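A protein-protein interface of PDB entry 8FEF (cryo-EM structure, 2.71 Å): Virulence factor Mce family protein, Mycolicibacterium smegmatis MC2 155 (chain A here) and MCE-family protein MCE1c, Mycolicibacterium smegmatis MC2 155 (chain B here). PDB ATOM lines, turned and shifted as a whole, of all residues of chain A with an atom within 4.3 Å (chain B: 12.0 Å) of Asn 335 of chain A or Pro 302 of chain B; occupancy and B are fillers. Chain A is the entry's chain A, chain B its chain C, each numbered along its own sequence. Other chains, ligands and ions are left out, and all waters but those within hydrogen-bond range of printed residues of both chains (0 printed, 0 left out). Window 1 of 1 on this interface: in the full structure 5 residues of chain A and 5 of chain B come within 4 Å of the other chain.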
ATOM      1  N   VAL A 333      -6.907  12.037  -3.466  1.00  0.00           N
ATOM      2  CA  VAL A 333      -7.053  13.390  -3.993  1.00  0.00           C
ATOM      3  C   VAL A 333      -6.839  14.398  -2.878  1.00  0.00           C
ATOM      4  O   VAL A 333      -7.200  14.156  -1.719  1.00  0.00           O
ATOM      5  CB  VAL A 333      -8.422  13.601  -4.667  1.00  0.00           C
ATOM      6  CG1 VAL A 333      -8.545  12.726  -5.869  1.00  0.00           C
ATOM      7  CG2 VAL A 333      -9.536  13.275  -3.705  1.00  0.00           C
ATOM      8  N   GLY A 334      -6.246  15.530  -3.227  1.00  0.00           N
ATOM      9  CA  GLY A 334      -6.027  16.585  -2.266  1.00  0.00           C
ATOM     10  C   GLY A 334      -7.317  17.274  -1.869  1.00  0.00           C
ATOM     11  O   GLY A 334      -8.389  17.057  -2.435  1.00  0.00           O
ATOM     12  N   ASN A 335      -7.200  18.121  -0.854  1.00  0.00           N
ATOM     13  CA  ASN A 335      -8.360  18.824  -0.333  1.00  0.00           C
ATOM     14  C   ASN A 335      -8.871  19.830  -1.362  1.00  0.00           C
ATOM     15  O   ASN A 335      -8.074  20.436  -2.084  1.00  0.00           O
ATOM     16  CB  ASN A 335      -8.005  19.538   0.968  1.00  0.00           C
ATOM     17  CG  ASN A 335      -7.466  18.593   2.017  1.00  0.00           C
ATOM     18  OD1 ASN A 335      -7.881  17.438   2.098  1.00  0.00           O
ATOM     19  ND2 ASN A 335      -6.531  19.076   2.824  1.00  0.00           N
ATOM     20  N   PRO A 336     -10.189  20.018  -1.458  1.00  0.00           N
ATOM     21  CA  PRO A 336     -10.734  20.959  -2.443  1.00  0.00           C
ATOM     22  C   PRO A 336     -10.262  22.380  -2.184  1.00  0.00           C
ATOM     23  O   PRO A 336      -9.864  22.745  -1.075  1.00  0.00           O
ATOM     24  CB  PRO A 336     -12.251  20.837  -2.252  1.00  0.00           C
ATOM     25  CG  PRO A 336     -12.450  19.518  -1.595  1.00  0.00           C
ATOM     26  CD  PRO A 336     -11.250  19.305  -0.730  1.00  0.00           C
ATOM     27  N   TYR A 337     -10.293  23.183  -3.243  1.00  0.00           N
ATOM     28  CA  TYR A 337      -9.897  24.578  -3.138  1.00  0.00           C
ATOM     29  C   TYR A 337     -10.877  25.343  -2.256  1.00  0.00           C
ATOM     30  O   TYR A 337     -12.092  25.257  -2.446  1.00  0.00           O
ATOM     31  CB  TYR A 337      -9.842  25.202  -4.530  1.00  0.00           C
ATOM     32  CG  TYR A 337      -8.717  24.686  -5.398  1.00  0.00           C
ATOM     33  CD1 TYR A 337      -7.451  24.466  -4.874  1.00  0.00           C
ATOM     34  CD2 TYR A 337      -8.926  24.409  -6.739  1.00  0.00           C
ATOM     35  CE1 TYR A 337      -6.424  23.993  -5.668  1.00  0.00           C
ATOM     36  CE2 TYR A 337      -7.908  23.936  -7.538  1.00  0.00           C
ATOM     37  CZ  TYR A 337      -6.659  23.731  -7.000  1.00  0.00           C
ATOM     38  OH  TYR A 337      -5.643  23.260  -7.798  1.00  0.00           O
ATOM     39  N   ILE A 380       0.095  22.477  -4.691  1.00  0.00           N
ATOM     40  CA  ILE A 380      -0.012  21.112  -4.185  1.00  0.00           C
ATOM     41  C   ILE A 380       1.297  20.759  -3.496  1.00  0.00           C
ATOM     42  O   ILE A 380       1.593  19.584  -3.259  1.00  0.00           O
ATOM     43  CB  ILE A 380      -0.344  20.097  -5.295  1.00  0.00           C
ATOM     44  CG1 ILE A 380       0.793  20.016  -6.312  1.00  0.00           C
ATOM     45  CG2 ILE A 380      -1.665  20.436  -5.966  1.00  0.00           C
ATOM     46  CD1 ILE A 380       0.591  18.955  -7.363  1.00  0.00           C
ATOM     47  N   TYR A 383       1.507  18.534   0.082  1.00  0.00           N
ATOM     48  CA  TYR A 383       1.067  17.141   0.117  1.00  0.00           C
ATOM     49  C   TYR A 383       2.274  16.200   0.141  1.00  0.00           C
ATOM     50  O   TYR A 383       2.516  15.421  -0.779  1.00  0.00           O
ATOM     51  CB  TYR A 383       0.154  16.844  -1.067  1.00  0.00           C
ATOM     52  CG  TYR A 383      -1.203  17.495  -0.968  1.00  0.00           C
ATOM     53  CD1 TYR A 383      -2.188  16.969  -0.148  1.00  0.00           C
ATOM     54  CD2 TYR A 383      -1.502  18.634  -1.701  1.00  0.00           C
ATOM     55  CE1 TYR A 383      -3.429  17.560  -0.056  1.00  0.00           C
ATOM     56  CE2 TYR A 383      -2.742  19.232  -1.615  1.00  0.00           C
ATOM     57  CZ  TYR A 383      -3.701  18.690  -0.791  1.00  0.00           C
ATOM     58  OH  TYR A 383      -4.939  19.279  -0.700  1.00  0.00           O
ATOM     59  N   GLY A 389      -8.653  13.234   4.592  1.00  0.00           N
ATOM     60  CA  GLY A 389      -9.281  14.394   3.993  1.00  0.00           C
ATOM     61  C   GLY A 389      -9.939  15.277   5.030  1.00  0.00           C
ATOM     62  O   GLY A 389     -10.741  14.795   5.834  1.00  0.00           O
ATOM     63  N   GLN A 390      -9.583  16.563   5.042  1.00  0.00           N
ATOM     64  CA  GLN A 390     -10.098  17.460   6.075  1.00  0.00           C
ATOM     65  C   GLN A 390     -11.616  17.589   6.017  1.00  0.00           C
ATOM     66  O   GLN A 390     -12.262  17.438   7.068  1.00  0.00           O
ATOM     67  CB  GLN A 390      -9.382  18.813   5.987  1.00  0.00           C
ATOM     68  CG  GLN A 390      -7.866  18.713   5.974  1.00  0.00           C
ATOM     69  CD  GLN A 390      -7.291  18.232   7.289  1.00  0.00           C
ATOM     70  OE1 GLN A 390      -7.929  18.337   8.335  1.00  0.00           O
ATOM     71  NE2 GLN A 390      -6.077  17.702   7.243  1.00  0.00           N
ATOM     72  N   PRO A 409      -2.721  21.427   4.873  1.00  0.00           N
ATOM     73  CA  PRO A 409      -2.931  20.003   5.127  1.00  0.00           C
ATOM     74  C   PRO A 409      -1.718  19.376   5.794  1.00  0.00           C
ATOM     75  O   PRO A 409      -0.603  19.881   5.680  1.00  0.00           O
ATOM     76  CB  PRO A 409      -3.146  19.428   3.727  1.00  0.00           C
ATOM     77  CG  PRO A 409      -2.376  20.332   2.842  1.00  0.00           C
ATOM     78  CD  PRO A 409      -2.480  21.702   3.446  1.00  0.00           C
ATOM     79  OXT PRO A 409      -1.825  18.356   6.467  1.00  0.00           O
ATOM     80  N   ALA B 295     -11.824  24.679 -19.070  1.00  0.00           N
ATOM     81  CA  ALA B 295     -10.963  24.910 -17.927  1.00  0.00           C
ATOM     82  C   ALA B 295     -11.766  24.875 -16.633  1.00  0.00           C
ATOM     83  O   ALA B 295     -11.210  25.034 -15.560  1.00  0.00           O
ATOM     84  CB  ALA B 295     -10.238  26.231 -18.069  1.00  0.00           C
ATOM     85  N   GLU B 296     -13.084  24.750 -16.752  1.00  0.00           N
ATOM     86  CA  GLU B 296     -13.988  24.666 -15.618  1.00  0.00           C
ATOM     87  C   GLU B 296     -13.790  23.384 -14.827  1.00  0.00           C
ATOM     88  O   GLU B 296     -13.876  23.382 -13.605  1.00  0.00           O
ATOM     89  CB  GLU B 296     -15.440  24.806 -16.069  1.00  0.00           C
ATOM     90  CG  GLU B 296     -16.222  25.830 -15.268  1.00  0.00           C
ATOM     91  CD  GLU B 296     -15.380  27.041 -14.908  1.00  0.00           C
ATOM     92  OE1 GLU B 296     -14.419  27.337 -15.641  1.00  0.00           O
ATOM     93  OE2 GLU B 296     -15.665  27.697 -13.888  1.00  0.00           O
ATOM     94  N   ALA B 297     -13.531  22.289 -15.535  1.00  0.00           N
ATOM     95  CA  ALA B 297     -13.347  20.982 -14.919  1.00  0.00           C
ATOM     96  C   ALA B 297     -12.166  20.986 -13.985  1.00  0.00           C
ATOM     97  O   ALA B 297     -12.227  20.417 -12.913  1.00  0.00           O
ATOM     98  CB  ALA B 297     -13.163  19.928 -15.986  1.00  0.00           C
ATOM     99  N   LEU B 298     -11.089  21.639 -14.381  1.00  0.00           N
ATOM    100  CA  LEU B 298      -9.897  21.726 -13.553  1.00  0.00           C
ATOM    101  C   LEU B 298     -10.084  22.497 -12.249  1.00  0.00           C
ATOM    102  O   LEU B 298      -9.384  22.254 -11.296  1.00  0.00           O
ATOM    103  CB  LEU B 298      -8.740  22.345 -14.328  1.00  0.00           C
ATOM    104  CG  LEU B 298      -8.394  21.872 -15.732  1.00  0.00           C
ATOM    105  CD1 LEU B 298      -6.987  22.328 -16.067  1.00  0.00           C
ATOM    106  CD2 LEU B 298      -8.492  20.366 -15.803  1.00  0.00           C
ATOM    107  N   ALA B 299     -10.995  23.461 -12.241  1.00  0.00           N
ATOM    108  CA  ALA B 299     -11.256  24.365 -11.112  1.00  0.00           C
ATOM    109  C   ALA B 299     -11.738  23.852  -9.752  1.00  0.00           C
ATOM    110  O   ALA B 299     -11.313  24.359  -8.727  1.00  0.00           O
ATOM    111  CB  ALA B 299     -12.164  25.486 -11.572  1.00  0.00           C
ATOM    112  N   SER B 300     -12.590  22.842  -9.722  1.00  0.00           N
ATOM    113  CA  SER B 300     -13.166  22.372  -8.457  1.00  0.00           C
ATOM    114  C   SER B 300     -12.193  21.909  -7.390  1.00  0.00           C
ATOM    115  O   SER B 300     -12.466  22.104  -6.232  1.00  0.00           O
ATOM    116  CB  SER B 300     -14.192  21.262  -8.702  1.00  0.00           C
ATOM    117  OG  SER B 300     -15.113  21.599  -9.729  1.00  0.00           O
ATOM    118  N   GLY B 301     -11.106  21.249  -7.763  1.00  0.00           N
ATOM    119  CA  GLY B 301     -10.116  20.740  -6.816  1.00  0.00           C
ATOM    120  C   GLY B 301      -8.779  20.559  -7.514  1.00  0.00           C
ATOM    121  O   GLY B 301      -8.637  20.963  -8.653  1.00  0.00           O
ATOM    122  N   PRO B 302      -7.761  19.998  -6.841  1.00  0.00           N
ATOM    123  CA  PRO B 302      -6.490  19.794  -7.560  1.00  0.00           C
ATOM    124  C   PRO B 302      -6.453  18.501  -8.395  1.00  0.00           C
ATOM    125  O   PRO B 302      -5.690  17.603  -8.088  1.00  0.00           O
ATOM    126  CB  PRO B 302      -5.467  19.706  -6.431  1.00  0.00           C
ATOM    127  CG  PRO B 302      -6.236  19.204  -5.269  1.00  0.00           C
ATOM    128  CD  PRO B 302      -7.655  19.669  -5.415  1.00  0.00           C
ATOM    129  N   TYR B 303      -7.267  18.457  -9.452  1.00  0.00           N
ATOM    130  CA  TYR B 303      -7.453  17.339 -10.377  1.00  0.00           C
ATOM    131  C   TYR B 303      -8.412  17.841 -11.455  1.00  0.00           C
ATOM    132  O   TYR B 303      -8.414  19.013 -11.756  1.00  0.00           O
ATOM    133  CB  TYR B 303      -8.093  16.148  -9.652  1.00  0.00           C
ATOM    134  CG  TYR B 303      -9.181  16.507  -8.653  1.00  0.00           C
ATOM    135  CD1 TYR B 303     -10.437  16.886  -9.072  1.00  0.00           C
ATOM    136  CD2 TYR B 303      -8.939  16.469  -7.294  1.00  0.00           C
ATOM    137  CE1 TYR B 303     -11.422  17.223  -8.172  1.00  0.00           C
ATOM    138  CE2 TYR B 303      -9.915  16.812  -6.387  1.00  0.00           C
ATOM    139  CZ  TYR B 303     -11.154  17.184  -6.837  1.00  0.00           C
ATOM    140  OH  TYR B 303     -12.132  17.520  -5.939  1.00  0.00           O
ATOM    141  N   PHE B 304      -9.185  16.955 -12.071  1.00  0.00           N
ATOM    142  CA  PHE B 304     -10.221  17.324 -13.025  1.00  0.00           C
ATOM    143  C   PHE B 304     -11.342  16.300 -12.969  1.00  0.00           C
ATOM    144  O   PHE B 304     -11.088  15.100 -12.854  1.00  0.00           O
ATOM    145  CB  PHE B 304      -9.668  17.443 -14.456  1.00  0.00           C
ATOM    146  CG  PHE B 304      -8.944  16.219 -14.942  1.00  0.00           C
ATOM    147  CD1 PHE B 304      -7.590  16.075 -14.728  1.00  0.00           C
ATOM    148  CD2 PHE B 304      -9.610  15.226 -15.637  1.00  0.00           C
ATOM    149  CE1 PHE B 304      -6.919  14.960 -15.178  1.00  0.00           C
ATOM    150  CE2 PHE B 304      -8.937  14.108 -16.087  1.00  0.00           C
ATOM    151  CZ  PHE B 304      -7.595  13.976 -15.857  1.00  0.00           C
ATOM    152  N   LYS B 305     -12.581  16.771 -13.035  1.00  0.00           N
ATOM    153  CA  LYS B 305     -13.707  15.853 -13.031  1.00  0.00           C
ATOM    154  C   LYS B 305     -13.822  15.140 -14.372  1.00  0.00           C
ATOM    155  O   LYS B 305     -13.530  15.705 -15.429  1.00  0.00           O
ATOM    156  CB  LYS B 305     -15.003  16.598 -12.726  1.00  0.00           C
ATOM    157  CG  LYS B 305     -14.979  17.380 -11.432  1.00  0.00           C
ATOM    158  CD  LYS B 305     -16.342  17.974 -11.137  1.00  0.00           C
ATOM    159  CE  LYS B 305     -16.273  18.928  -9.966  1.00  0.00           C
ATOM    160  NZ  LYS B 305     -15.579  18.301  -8.815  1.00  0.00           N
ATOM    161  N   VAL B 306     -14.245  13.881 -14.321  1.00  0.00           N
ATOM    162  CA  VAL B 306     -14.463  13.068 -15.512  1.00  0.00           C
ATOM    163  C   VAL B 306     -15.743  12.268 -15.337  1.00  0.00           C
ATOM    164  O   VAL B 306     -16.021  11.747 -14.252  1.00  0.00           O
ATOM    165  CB  VAL B 306     -13.275  12.128 -15.800  1.00  0.00           C
ATOM    166  CG1 VAL B 306     -12.134  12.898 -16.400  1.00  0.00           C
ATOM    167  CG2 VAL B 306     -12.822  11.430 -14.533  1.00  0.00           C
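The side-chain hydroxyl (OH) of Tyr 383 of chain A is in hydrogen-bond range of the backbone NH (N) of Asn 335 of chain A, 2.5 Å away. The side-chain hydroxyl (OG) of Ser 300 of chain B sits close to the side-chain amino group (NZ) of Lys 305 of chain B, 3.5 Å away.
Val 333 of chain A touches one residue of chain B. Of the printed residues of chain B, Gly 334 of chain A touches Pro 302 (3.99 Å). Asn 335 of chain A touches just one residue of chain B: Pro 302. No residue of chain B comes within 4 Å of Pro 336 of chain A. Tyr 337 of chain A touches just these residues of chain B: Ala 299, Ser 300, Gly 301 and Pro 302. Ile 380 of chain A touches just one residue of chain B: Pro 302. No residue of chain B comes within 4 Å of Gly 389 of chain A. No residue of chain B comes within 4 Å of Gln 390 of chain A. Of the printed residues of chain A, Ala 299 of chain B touches Tyr 337. Of the printed residues of chain A, Ser 300 of chain B touches Tyr 337 (3.8 Å). Printed residues of chain A within 4 Å of Pro 302 of chain B: Gly 334, Asn 335, Tyr 337 and Ile 380. The nearest residue of chain B that does not touch Asn 335 of chain A is Gly 301 of chain B (5.2 Å). The nearest printed residue of chain A that does not touch Pro 302 of chain B is Pro 336 of chain A (4.5 Å).
Among the printed residues, pairs that only touch across the chains: Val 333 of chain A with Tyr 303 of chain B, Gly 334 of chain A with Pro 302 of chain B, Asn 335 of chain A with Pro 302 of chain B, Tyr 337 of chain A with Ala 299 of chain B, Tyr 337 of chain A with Ser 300 of chain B, Tyr 337 of chain A with Gly 301 of chain B, Tyr 337 of chain A with Pro 302 of chain B and Ile 380 of chain A with Pro 302 of chain B.
Hydrophobic or aromatic side chains of chain A within 4 Å of the printed part of chain B: Val 333, Tyr 337 and Ile 380. Of the 12 printed residues of chain B, 5 touch a printed residue of chain A. Printed residues of chain B that touch a printed residue of chain A: Ala 299, Ser 300, Gly 301, Pro 302 and Tyr 303. Among the printed residues, 8 pairs touch across the chains. Among the printed residues, no Asp or Glu carboxylate lies within 4 Å of a Lys or Arg side-chain nitrogen of the other chain.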
